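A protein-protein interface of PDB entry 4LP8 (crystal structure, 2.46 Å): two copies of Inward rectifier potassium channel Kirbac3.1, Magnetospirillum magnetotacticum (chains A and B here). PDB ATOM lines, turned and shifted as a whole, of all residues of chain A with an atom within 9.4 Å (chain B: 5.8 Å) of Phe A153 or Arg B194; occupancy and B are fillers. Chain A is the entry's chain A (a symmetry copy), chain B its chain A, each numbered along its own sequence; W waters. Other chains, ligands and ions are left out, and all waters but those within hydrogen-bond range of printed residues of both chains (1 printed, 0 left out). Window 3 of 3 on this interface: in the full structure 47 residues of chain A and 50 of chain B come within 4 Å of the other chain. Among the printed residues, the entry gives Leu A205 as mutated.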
ATOM      1  N   VAL A 149      -5.020 -31.217 -19.354  1.00  0.00           N
ATOM      2  CA  VAL A 149      -3.817 -32.053 -19.303  1.00  0.00           C
ATOM      3  C   VAL A 149      -2.632 -31.218 -18.851  1.00  0.00           C
ATOM      4  O   VAL A 149      -2.673 -30.010 -18.957  1.00  0.00           O
ATOM      5  CB  VAL A 149      -3.530 -32.775 -20.654  1.00  0.00           C
ATOM      6  CG1 VAL A 149      -4.636 -33.750 -21.012  1.00  0.00           C
ATOM      7  CG2 VAL A 149      -3.265 -31.805 -21.794  1.00  0.00           C
ATOM      8  N   ILE A 150      -1.587 -31.845 -18.346  1.00  0.00           N
ATOM      9  CA  ILE A 150      -0.336 -31.158 -18.024  1.00  0.00           C
ATOM     10  C   ILE A 150       0.743 -31.995 -18.646  1.00  0.00           C
ATOM     11  O   ILE A 150       0.991 -33.108 -18.186  1.00  0.00           O
ATOM     12  CB  ILE A 150      -0.058 -30.828 -16.528  1.00  0.00           C
ATOM     13  CG1 ILE A 150      -1.115 -29.854 -15.969  1.00  0.00           C
ATOM     14  CG2 ILE A 150       1.366 -30.272 -16.358  1.00  0.00           C
ATOM     15  CD1 ILE A 150      -0.884 -29.260 -14.552  1.00  0.00           C
ATOM     16  N   SER A 151       1.353 -31.503 -19.720  1.00  0.00           N
ATOM     17  CA  SER A 151       2.438 -32.225 -20.381  1.00  0.00           C
ATOM     18  C   SER A 151       3.398 -31.229 -21.021  1.00  0.00           C
ATOM     19  O   SER A 151       3.057 -30.053 -21.139  1.00  0.00           O
ATOM     20  CB  SER A 151       1.885 -33.210 -21.409  1.00  0.00           C
ATOM     21  OG  SER A 151       1.061 -32.573 -22.376  1.00  0.00           O
ATOM     22  N   ASP A 152       4.592 -31.689 -21.430  1.00  0.00           N
ATOM     23  CA  ASP A 152       5.594 -30.825 -22.036  1.00  0.00           C
ATOM     24  C   ASP A 152       5.221 -30.468 -23.476  1.00  0.00           C
ATOM     25  O   ASP A 152       4.723 -31.303 -24.230  1.00  0.00           O
ATOM     26  CB  ASP A 152       6.992 -31.457 -21.950  1.00  0.00           C
ATOM     27  CG  ASP A 152       7.513 -31.651 -20.522  1.00  0.00           C
ATOM     28  OD1 ASP A 152       6.691 -31.600 -19.568  1.00  0.00           O
ATOM     29  OD2 ASP A 152       8.724 -31.868 -20.358  1.00  0.00           O
ATOM     30  N   PHE A 153       5.371 -29.175 -23.800  1.00  0.00           N
ATOM     31  CA  PHE A 153       5.150 -28.562 -25.109  1.00  0.00           C
ATOM     32  C   PHE A 153       6.236 -27.508 -25.280  1.00  0.00           C
ATOM     33  O   PHE A 153       6.371 -26.635 -24.409  1.00  0.00           O
ATOM     34  CB  PHE A 153       3.734 -27.961 -25.229  1.00  0.00           C
ATOM     35  CG  PHE A 153       3.462 -27.375 -26.593  1.00  0.00           C
ATOM     36  CD1 PHE A 153       3.068 -28.186 -27.649  1.00  0.00           C
ATOM     37  CD2 PHE A 153       3.625 -26.013 -26.829  1.00  0.00           C
ATOM     38  CE1 PHE A 153       2.841 -27.645 -28.919  1.00  0.00           C
ATOM     39  CE2 PHE A 153       3.400 -25.474 -28.101  1.00  0.00           C
ATOM     40  CZ  PHE A 153       3.007 -26.293 -29.135  1.00  0.00           C
ATOM     41  N   GLU A 154       7.048 -27.620 -26.361  1.00  0.00           N
ATOM     42  CA  GLU A 154       8.202 -26.753 -26.646  1.00  0.00           C
ATOM     43  C   GLU A 154       9.136 -26.716 -25.422  1.00  0.00           C
ATOM     44  O   GLU A 154       9.520 -25.641 -24.950  1.00  0.00           O
ATOM     45  CB  GLU A 154       7.786 -25.329 -27.096  1.00  0.00           C
ATOM     46  CG  GLU A 154       6.807 -25.259 -28.263  1.00  0.00           C
ATOM     47  CD  GLU A 154       7.239 -25.782 -29.620  1.00  0.00           C
ATOM     48  OE1 GLU A 154       7.833 -26.885 -29.690  1.00  0.00           O
ATOM     49  OE2 GLU A 154       6.921 -25.110 -30.629  1.00  0.00           O
ATOM     50  N   GLY A 155       9.426 -27.913 -24.898  1.00  0.00           N
ATOM     51  CA  GLY A 155      10.312 -28.158 -23.758  1.00  0.00           C
ATOM     52  C   GLY A 155       9.948 -27.486 -22.447  1.00  0.00           C
ATOM     53  O   GLY A 155      10.829 -27.215 -21.628  1.00  0.00           O
ATOM     54  N   LYS A 156       8.654 -27.233 -22.222  1.00  0.00           N
ATOM     55  CA  LYS A 156       8.169 -26.594 -20.994  1.00  0.00           C
ATOM     56  C   LYS A 156       6.866 -27.269 -20.549  1.00  0.00           C
ATOM     57  O   LYS A 156       6.043 -27.539 -21.417  1.00  0.00           O
ATOM     58  CB  LYS A 156       7.961 -25.085 -21.252  1.00  0.00           C
ATOM     59  CG  LYS A 156       7.562 -24.258 -20.028  1.00  0.00           C
ATOM     60  CD  LYS A 156       8.699 -23.400 -19.509  1.00  0.00           C
ATOM     61  CE  LYS A 156       8.725 -21.976 -20.041  1.00  0.00           C
ATOM     62  NZ  LYS A 156       9.174 -21.875 -21.455  1.00  0.00           N
ATOM     63  N   PRO A 157       6.632 -27.559 -19.241  1.00  0.00           N
ATOM     64  CA  PRO A 157       5.339 -28.157 -18.847  1.00  0.00           C
ATOM     65  C   PRO A 157       4.212 -27.156 -19.114  1.00  0.00           C
ATOM     66  O   PRO A 157       4.349 -25.969 -18.803  1.00  0.00           O
ATOM     67  CB  PRO A 157       5.514 -28.479 -17.354  1.00  0.00           C
ATOM     68  CG  PRO A 157       6.951 -28.272 -17.055  1.00  0.00           C
ATOM     69  CD  PRO A 157       7.483 -27.306 -18.061  1.00  0.00           C
ATOM     70  N   THR A 158       3.127 -27.623 -19.756  1.00  0.00           N
ATOM     71  CA  THR A 158       2.035 -26.771 -20.222  1.00  0.00           C
ATOM     72  C   THR A 158       0.678 -27.310 -19.804  1.00  0.00           C
ATOM     73  O   THR A 158       0.405 -28.492 -19.976  1.00  0.00           O
ATOM     74  CB  THR A 158       2.156 -26.651 -21.764  1.00  0.00           C
ATOM     75  OG1 THR A 158       3.459 -26.132 -22.098  1.00  0.00           O
ATOM     76  CG2 THR A 158       1.097 -25.775 -22.385  1.00  0.00           C
ATOM     77  N   LEU A 159      -0.175 -26.428 -19.262  1.00  0.00           N
ATOM     78  CA  LEU A 159      -1.558 -26.761 -18.898  1.00  0.00           C
ATOM     79  C   LEU A 159      -2.419 -26.570 -20.145  1.00  0.00           C
ATOM     80  O   LEU A 159      -2.299 -25.550 -20.815  1.00  0.00           O
ATOM     81  CB  LEU A 159      -2.055 -25.870 -17.730  1.00  0.00           C
ATOM     82  CG  LEU A 159      -3.505 -26.066 -17.239  1.00  0.00           C
ATOM     83  CD1 LEU A 159      -3.667 -27.387 -16.485  1.00  0.00           C
ATOM     84  CD2 LEU A 159      -3.884 -24.963 -16.283  1.00  0.00           C
ATOM     85  N   MET A 160      -3.254 -27.553 -20.487  1.00  0.00           N
ATOM     86  CA  MET A 160      -4.074 -27.488 -21.700  1.00  0.00           C
ATOM     87  C   MET A 160      -5.459 -28.002 -21.504  1.00  0.00           C
ATOM     88  O   MET A 160      -5.691 -28.887 -20.705  1.00  0.00           O
ATOM     89  CB  MET A 160      -3.427 -28.308 -22.846  1.00  0.00           C
ATOM     90  CG  MET A 160      -1.946 -28.047 -23.050  1.00  0.00           C
ATOM     91  SD  MET A 160      -1.273 -28.944 -24.452  1.00  0.00           S
ATOM     92  CE  MET A 160       0.331 -29.343 -23.858  1.00  0.00           C
ATOM     93  N   LEU A 200      -2.161 -17.339 -21.394  1.00  0.00           N
ATOM     94  CA  LEU A 200      -2.219 -18.332 -22.448  1.00  0.00           C
ATOM     95  C   LEU A 200      -1.277 -17.976 -23.570  1.00  0.00           C
ATOM     96  O   LEU A 200      -1.010 -16.789 -23.793  1.00  0.00           O
ATOM     97  CB  LEU A 200      -3.665 -18.433 -22.970  1.00  0.00           C
ATOM     98  CG  LEU A 200      -4.756 -18.708 -21.943  1.00  0.00           C
ATOM     99  CD1 LEU A 200      -6.140 -18.598 -22.586  1.00  0.00           C
ATOM    100  CD2 LEU A 200      -4.551 -20.034 -21.258  1.00  0.00           C
ATOM    101  N   THR A 201      -0.800 -18.995 -24.310  1.00  0.00           N
ATOM    102  CA  THR A 201       0.073 -18.808 -25.472  1.00  0.00           C
ATOM    103  C   THR A 201      -0.701 -18.004 -26.543  1.00  0.00           C
ATOM    104  O   THR A 201      -0.130 -17.134 -27.215  1.00  0.00           O
ATOM    105  CB  THR A 201       0.543 -20.166 -25.976  1.00  0.00           C
ATOM    106  OG1 THR A 201       1.529 -20.640 -25.077  1.00  0.00           O
ATOM    107  CG2 THR A 201       1.139 -20.107 -27.366  1.00  0.00           C
ATOM    108  N   ARG A 202      -2.007 -18.334 -26.681  1.00  0.00           N
ATOM    109  CA  ARG A 202      -2.970 -17.713 -27.576  1.00  0.00           C
ATOM    110  C   ARG A 202      -4.285 -17.631 -26.831  1.00  0.00           C
ATOM    111  O   ARG A 202      -4.807 -18.666 -26.420  1.00  0.00           O
ATOM    112  CB  ARG A 202      -3.112 -18.504 -28.889  1.00  0.00           C
ATOM    113  CG  ARG A 202      -4.236 -17.953 -29.773  1.00  0.00           C
ATOM    114  CD  ARG A 202      -4.319 -18.573 -31.142  1.00  0.00           C
ATOM    115  NE  ARG A 202      -3.186 -18.194 -31.982  1.00  0.00           N
ATOM    116  CZ  ARG A 202      -3.136 -17.120 -32.762  1.00  0.00           C
ATOM    117  NH1 ARG A 202      -4.160 -16.279 -32.818  1.00  0.00           N
ATOM    118  NH2 ARG A 202      -2.053 -16.867 -33.478  1.00  0.00           N
ATOM    119  N   LEU A 205      -8.353 -16.175 -31.038  1.00  0.00           N
ATOM    120  CA  LEU A 205      -8.369 -16.889 -32.294  1.00  0.00           C
ATOM    121  C   LEU A 205      -9.338 -16.114 -33.189  1.00  0.00           C
ATOM    122  O   LEU A 205     -10.545 -16.064 -32.880  1.00  0.00           O
ATOM    123  CB  LEU A 205      -8.789 -18.333 -32.047  1.00  0.00           C
ATOM    124  CG  LEU A 205      -8.605 -19.277 -33.225  1.00  0.00           C
ATOM    125  CD1 LEU A 205      -7.131 -19.408 -33.592  1.00  0.00           C
ATOM    126  CD2 LEU A 205      -9.233 -20.634 -32.914  1.00  0.00           C
ATOM    127  N   THR A 213      -6.894 -25.917 -29.078  1.00  0.00           N
ATOM    128  CA  THR A 213      -6.220 -26.341 -27.835  1.00  0.00           C
ATOM    129  C   THR A 213      -5.608 -25.110 -27.220  1.00  0.00           C
ATOM    130  O   THR A 213      -4.838 -24.401 -27.864  1.00  0.00           O
ATOM    131  CB  THR A 213      -5.197 -27.465 -28.039  1.00  0.00           C
ATOM    132  OG1 THR A 213      -5.839 -28.499 -28.767  1.00  0.00           O
ATOM    133  CG2 THR A 213      -4.683 -28.038 -26.700  1.00  0.00           C
ATOM    134  N   VAL A 214      -6.038 -24.820 -26.000  1.00  0.00           N
ATOM    135  CA  VAL A 214      -5.646 -23.662 -25.184  1.00  0.00           C
ATOM    136  C   VAL A 214      -4.463 -24.091 -24.303  1.00  0.00           C
ATOM    137  O   VAL A 214      -4.492 -25.174 -23.727  1.00  0.00           O
ATOM    138  CB  VAL A 214      -6.869 -23.202 -24.379  1.00  0.00           C
ATOM    139  CG1 VAL A 214      -6.545 -21.980 -23.568  1.00  0.00           C
ATOM    140  CG2 VAL A 214      -8.042 -22.929 -25.301  1.00  0.00           C
ATOM    141  N   MET A 215      -3.396 -23.294 -24.274  1.00  0.00           N
ATOM    142  CA  MET A 215      -2.185 -23.683 -23.563  1.00  0.00           C
ATOM    143  C   MET A 215      -1.715 -22.650 -22.598  1.00  0.00           C
ATOM    144  O   MET A 215      -1.556 -21.495 -22.971  1.00  0.00           O
ATOM    145  CB  MET A 215      -1.059 -23.942 -24.572  1.00  0.00           C
ATOM    146  CG  MET A 215      -1.235 -25.199 -25.384  1.00  0.00           C
ATOM    147  SD  MET A 215      -0.218 -25.109 -26.853  1.00  0.00           S
ATOM    148  CE  MET A 215      -0.417 -26.719 -27.421  1.00  0.00           C
ATOM    149  N   HIS A 216      -1.427 -23.070 -21.369  1.00  0.00           N
ATOM    150  CA  HIS A 216      -0.837 -22.211 -20.347  1.00  0.00           C
ATOM    151  C   HIS A 216       0.570 -22.768 -20.005  1.00  0.00           C
ATOM    152  O   HIS A 216       0.697 -23.757 -19.270  1.00  0.00           O
ATOM    153  CB  HIS A 216      -1.739 -22.061 -19.103  1.00  0.00           C
ATOM    154  CG  HIS A 216      -1.009 -21.497 -17.920  1.00  0.00           C
ATOM    155  ND1 HIS A 216      -0.498 -20.192 -17.928  1.00  0.00           N
ATOM    156  CD2 HIS A 216      -0.646 -22.100 -16.762  1.00  0.00           C
ATOM    157  CE1 HIS A 216       0.128 -20.050 -16.768  1.00  0.00           C
ATOM    158  NE2 HIS A 216       0.055 -21.169 -16.029  1.00  0.00           N
ATOM    159  N   PRO A 217       1.646 -22.165 -20.559  1.00  0.00           N
ATOM    160  CA  PRO A 217       3.004 -22.637 -20.205  1.00  0.00           C
ATOM    161  C   PRO A 217       3.290 -22.378 -18.721  1.00  0.00           C
ATOM    162  O   PRO A 217       3.071 -21.263 -18.240  1.00  0.00           O
ATOM    163  CB  PRO A 217       3.931 -21.842 -21.126  1.00  0.00           C
ATOM    164  CG  PRO A 217       3.012 -21.139 -22.135  1.00  0.00           C
ATOM    165  CD  PRO A 217       1.693 -20.984 -21.450  1.00  0.00           C
ATOM    166  N   ILE A 218       3.657 -23.452 -17.974  1.00  0.00           N
ATOM    167  CA  ILE A 218       3.911 -23.369 -16.544  1.00  0.00           C
ATOM    168  C   ILE A 218       5.365 -22.923 -16.359  1.00  0.00           C
ATOM    169  O   ILE A 218       6.268 -23.747 -16.190  1.00  0.00           O
ATOM    170  CB  ILE A 218       3.532 -24.671 -15.755  1.00  0.00           C
ATOM    171  CG1 ILE A 218       2.054 -25.099 -16.027  1.00  0.00           C
ATOM    172  CG2 ILE A 218       3.758 -24.486 -14.249  1.00  0.00           C
ATOM    173  CD1 ILE A 218       1.715 -26.541 -15.708  1.00  0.00           C
ATOM    174  N   GLY A 269      -0.642 -36.312 -19.441  1.00  0.00           N
ATOM    175  CA  GLY A 269      -1.469 -36.657 -20.585  1.00  0.00           C
ATOM    176  C   GLY A 269      -1.374 -35.704 -21.755  1.00  0.00           C
ATOM    177  O   GLY A 269      -1.051 -34.531 -21.573  1.00  0.00           O
ATOM    178  N   HIS A 270      -1.658 -36.207 -22.975  1.00  0.00           N
ATOM    179  CA  HIS A 270      -1.693 -35.332 -24.139  1.00  0.00           C
ATOM    180  C   HIS A 270      -2.963 -35.632 -24.965  1.00  0.00           C
ATOM    181  O   HIS A 270      -3.458 -36.753 -24.994  1.00  0.00           O
ATOM    182  CB  HIS A 270      -0.388 -35.348 -24.969  1.00  0.00           C
ATOM    183  CG  HIS A 270      -0.046 -36.646 -25.632  1.00  0.00           C
ATOM    184  ND1 HIS A 270      -0.509 -36.950 -26.899  1.00  0.00           N
ATOM    185  CD2 HIS A 270       0.782 -37.634 -25.219  1.00  0.00           C
ATOM    186  CE1 HIS A 270       0.011 -38.129 -27.195  1.00  0.00           C
ATOM    187  NE2 HIS A 270       0.798 -38.576 -26.215  1.00  0.00           N
ATOM    188  N   LEU B 180      -0.687 -16.276 -39.909  1.00  0.00           N
ATOM    189  CA  LEU B 180      -0.012 -17.295 -40.697  1.00  0.00           C
ATOM    190  C   LEU B 180      -0.432 -18.626 -40.127  1.00  0.00           C
ATOM    191  O   LEU B 180      -0.486 -18.785 -38.898  1.00  0.00           O
ATOM    192  CB  LEU B 180       1.533 -17.132 -40.642  1.00  0.00           C
ATOM    193  CG  LEU B 180       2.427 -18.313 -41.098  1.00  0.00           C
ATOM    194  CD1 LEU B 180       2.371 -18.529 -42.592  1.00  0.00           C
ATOM    195  CD2 LEU B 180       3.874 -18.112 -40.659  1.00  0.00           C
ATOM    196  N   VAL B 181      -0.741 -19.581 -41.012  1.00  0.00           N
ATOM    197  CA  VAL B 181      -1.143 -20.929 -40.652  1.00  0.00           C
ATOM    198  C   VAL B 181      -0.233 -21.853 -41.445  1.00  0.00           C
ATOM    199  O   VAL B 181      -0.282 -21.858 -42.678  1.00  0.00           O
ATOM    200  CB  VAL B 181      -2.661 -21.222 -40.864  1.00  0.00           C
ATOM    201  CG1 VAL B 181      -3.056 -22.566 -40.255  1.00  0.00           C
ATOM    202  CG2 VAL B 181      -3.539 -20.101 -40.296  1.00  0.00           C
ATOM    203  N   ARG B 182       0.655 -22.575 -40.739  1.00  0.00           N
ATOM    204  CA  ARG B 182       1.572 -23.497 -41.390  1.00  0.00           C
ATOM    205  C   ARG B 182       1.667 -24.801 -40.618  1.00  0.00           C
ATOM    206  O   ARG B 182       1.285 -24.854 -39.445  1.00  0.00           O
ATOM    207  CB  ARG B 182       2.954 -22.872 -41.570  1.00  0.00           C
ATOM    208  CG  ARG B 182       3.708 -22.609 -40.281  1.00  0.00           C
ATOM    209  CD  ARG B 182       5.100 -22.153 -40.599  1.00  0.00           C
ATOM    210  NE  ARG B 182       5.814 -21.788 -39.381  1.00  0.00           N
ATOM    211  CZ  ARG B 182       6.687 -20.791 -39.297  1.00  0.00           C
ATOM    212  NH1 ARG B 182       6.955 -20.043 -40.360  1.00  0.00           N
ATOM    213  NH2 ARG B 182       7.305 -20.538 -38.153  1.00  0.00           N
ATOM    214  N   SER B 183       2.166 -25.850 -41.287  1.00  0.00           N
ATOM    215  CA  SER B 183       2.392 -27.176 -40.694  1.00  0.00           C
ATOM    216  C   SER B 183       3.747 -27.161 -40.030  1.00  0.00           C
ATOM    217  O   SER B 183       4.693 -26.624 -40.602  1.00  0.00           O
ATOM    218  CB  SER B 183       2.306 -28.265 -41.753  1.00  0.00           C
ATOM    219  OG  SER B 183       1.020 -28.241 -42.351  1.00  0.00           O
ATOM    220  N   GLU B 184       3.830 -27.654 -38.791  1.00  0.00           N
ATOM    221  CA  GLU B 184       5.072 -27.640 -38.013  1.00  0.00           C
ATOM    222  C   GLU B 184       5.297 -28.954 -37.266  1.00  0.00           C
ATOM    223  O   GLU B 184       4.344 -29.692 -37.001  1.00  0.00           O
ATOM    224  CB  GLU B 184       5.056 -26.484 -37.001  1.00  0.00           C
ATOM    225  CG  GLU B 184       5.285 -25.103 -37.596  1.00  0.00           C
ATOM    226  CD  GLU B 184       5.555 -24.001 -36.588  1.00  0.00           C
ATOM    227  OE1 GLU B 184       5.081 -24.110 -35.435  1.00  0.00           O
ATOM    228  OE2 GLU B 184       6.246 -23.024 -36.952  1.00  0.00           O
ATOM    229  N   SER B 186       6.720 -30.311 -33.728  1.00  0.00           N
ATOM    230  CA  SER B 186       7.027 -29.925 -32.346  1.00  0.00           C
ATOM    231  C   SER B 186       8.271 -30.667 -31.826  1.00  0.00           C
ATOM    232  O   SER B 186       8.664 -31.694 -32.393  1.00  0.00           O
ATOM    233  CB  SER B 186       5.829 -30.190 -31.437  1.00  0.00           C
ATOM    234  OG  SER B 186       6.092 -29.786 -30.102  1.00  0.00           O
ATOM    235  N   PHE B 192       1.606 -30.601 -36.620  1.00  0.00           N
ATOM    236  CA  PHE B 192       0.371 -29.833 -36.399  1.00  0.00           C
ATOM    237  C   PHE B 192       0.369 -28.487 -37.120  1.00  0.00           C
ATOM    238  O   PHE B 192       1.431 -27.903 -37.349  1.00  0.00           O
ATOM    239  CB  PHE B 192       0.169 -29.584 -34.882  1.00  0.00           C
ATOM    240  CG  PHE B 192       1.144 -28.635 -34.209  1.00  0.00           C
ATOM    241  CD1 PHE B 192       2.449 -29.028 -33.929  1.00  0.00           C
ATOM    242  CD2 PHE B 192       0.738 -27.369 -33.801  1.00  0.00           C
ATOM    243  CE1 PHE B 192       3.347 -28.154 -33.302  1.00  0.00           C
ATOM    244  CE2 PHE B 192       1.633 -26.501 -33.157  1.00  0.00           C
ATOM    245  CZ  PHE B 192       2.936 -26.896 -32.922  1.00  0.00           C
ATOM    246  N   ARG B 193      -0.831 -27.968 -37.418  1.00  0.00           N
ATOM    247  CA  ARG B 193      -1.002 -26.643 -38.010  1.00  0.00           C
ATOM    248  C   ARG B 193      -0.880 -25.588 -36.904  1.00  0.00           C
ATOM    249  O   ARG B 193      -1.674 -25.608 -35.950  1.00  0.00           O
ATOM    250  CB  ARG B 193      -2.365 -26.503 -38.720  1.00  0.00           C
ATOM    251  CG  ARG B 193      -2.569 -27.358 -39.957  1.00  0.00           C
ATOM    252  CD  ARG B 193      -1.790 -26.855 -41.146  1.00  0.00           C
ATOM    253  NE  ARG B 193      -2.340 -25.628 -41.727  1.00  0.00           N
ATOM    254  CZ  ARG B 193      -1.913 -25.109 -42.872  1.00  0.00           C
ATOM    255  NH1 ARG B 193      -0.948 -25.705 -43.558  1.00  0.00           N
ATOM    256  NH2 ARG B 193      -2.454 -23.998 -43.345  1.00  0.00           N
ATOM    257  N   ARG B 194       0.119 -24.694 -36.996  1.00  0.00           N
ATOM    258  CA  ARG B 194       0.248 -23.659 -35.974  1.00  0.00           C
ATOM    259  C   ARG B 194      -0.222 -22.307 -36.528  1.00  0.00           C
ATOM    260  O   ARG B 194      -0.033 -22.008 -37.718  1.00  0.00           O
ATOM    261  CB  ARG B 194       1.673 -23.567 -35.394  1.00  0.00           C
ATOM    262  CG  ARG B 194       1.680 -22.965 -33.982  1.00  0.00           C
ATOM    263  CD  ARG B 194       3.041 -22.994 -33.321  1.00  0.00           C
ATOM    264  NE  ARG B 194       2.981 -22.647 -31.899  1.00  0.00           N
ATOM    265  CZ  ARG B 194       4.016 -22.711 -31.065  1.00  0.00           C
ATOM    266  NH1 ARG B 194       5.202 -23.119 -31.501  1.00  0.00           N
ATOM    267  NH2 ARG B 194       3.871 -22.375 -29.790  1.00  0.00           N
ATOM    268  N   PHE B 195      -0.846 -21.507 -35.639  1.00  0.00           N
ATOM    269  CA  PHE B 195      -1.363 -20.177 -35.930  1.00  0.00           C
ATOM    270  C   PHE B 195      -0.444 -19.113 -35.329  1.00  0.00           C
ATOM    271  O   PHE B 195      -0.303 -19.024 -34.105  1.00  0.00           O
ATOM    272  CB  PHE B 195      -2.794 -20.032 -35.405  1.00  0.00           C
ATOM    273  CG  PHE B 195      -3.850 -20.800 -36.172  1.00  0.00           C
ATOM    274  CD1 PHE B 195      -3.766 -22.185 -36.317  1.00  0.00           C
ATOM    275  CD2 PHE B 195      -4.970 -20.152 -36.676  1.00  0.00           C
ATOM    276  CE1 PHE B 195      -4.758 -22.895 -36.997  1.00  0.00           C
ATOM    277  CE2 PHE B 195      -5.955 -20.860 -37.356  1.00  0.00           C
ATOM    278  CZ  PHE B 195      -5.842 -22.224 -37.516  1.00  0.00           C
ATOM    279  N   HIS B 196       0.207 -18.335 -36.208  1.00  0.00           N
ATOM    280  CA  HIS B 196       1.120 -17.273 -35.810  1.00  0.00           C
ATOM    281  C   HIS B 196       0.497 -15.933 -36.066  1.00  0.00           C
ATOM    282  O   HIS B 196       0.102 -15.670 -37.192  1.00  0.00           O
ATOM    283  CB  HIS B 196       2.445 -17.388 -36.573  1.00  0.00           C
ATOM    284  CG  HIS B 196       3.153 -18.676 -36.330  1.00  0.00           C
ATOM    285  ND1 HIS B 196       3.819 -18.915 -35.148  1.00  0.00           N
ATOM    286  CD2 HIS B 196       3.222 -19.784 -37.106  1.00  0.00           C
ATOM    287  CE1 HIS B 196       4.286 -20.149 -35.247  1.00  0.00           C
ATOM    288  NE2 HIS B 196       3.963 -20.707 -36.411  1.00  0.00           N
HETATM  289  O   HOH W   1       0.001 -18.348 -31.069  1.00  0.00           O
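The backbone carbonyl oxygen of Phe B195 sits at hydrogen-bond distance from the guanidinium group of Arg A202 (2.8 Å).
OG of Ser B186 is in hydrogen-bond range of OE1 of Glu A154, 3.4 Å away.
The guanidinium group (NH1) of Arg B194 is in salt-bridge range of the side-chain carboxylate (OE2) of Glu A154 (2.8 Å).
The backbone carbonyl oxygen (O) of Arg B182 is in hydrogen-bond range of the backbone NH (N) of Arg B194.
OE2 of Glu B184 lies within hydrogen-bond range of NE2 of His B196 (3.3 Å).
The backbone carbonyl oxygen of Leu B180 lies within hydrogen-bond range of the backbone NH of His B196 (2.8 Å).
The backbone NH (N) of Glu B184 is in hydrogen-bond range of the backbone carbonyl oxygen (O) of Phe B192 (2.8 Å).
Among the printed residues, merely in contact across the chains: Phe A153 with Arg B194, Arg A202 with His B196, Phe A153 with Phe B192 and Leu A205 with Phe B195.
Phe A153 touches two residues of chain B.
Of the printed residues of chain A, Phe B195 touches Arg A202 (2.8 Å) and Leu A205 (3.8 Å).
Printed residues of chain B within 4 Å of Glu A154: Ser B186 and Arg B194.
Printed residues of chain B within 4 Å of Leu A205: Phe B195 (3.8 Å).
Printed residues of chain A within 4 Å of Ser B186: Glu A154 (3.4 Å).
Printed residues of chain A within 4 Å of Phe B192: Phe A153 (3.8 Å).
Leu A200 touches none of the printed residues of chain B.
Thr A201 touches none of the printed residues of chain B.
The nearest residue of chain B that does not touch Phe A153 is Ser B186 (4.1 Å).
The nearest residue of chain A that does not touch Arg B194 is Thr A201 (4.3 Å).
Of the 11 printed residues of chain B, 5 touch a printed residue of chain A.
Of the 24 printed residues of chain A, 4 touch a printed residue of chain B.
Printed residues of chain A that touch a printed residue of chain B: Phe A153, Glu A154, Arg A202 and Leu A205.
Hydrophobic or aromatic side chains of chain A that line the printed part of chain B: Phe A153 and Leu A205.
Along chain A the printed residues that touch a printed residue of chain B span positions 153 to 205.
Among the printed residues, 7 pairs touch across the chains.
No position is printed for both chains.
Of the 7 pairs that touch across the chains among the printed residues, none has its exchanged pair printed and touching as well.
Water W1 lies within hydrogen-bond range of O of Phe B195 (3.1 Å) and NE of Arg A202 (3.3 Å).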
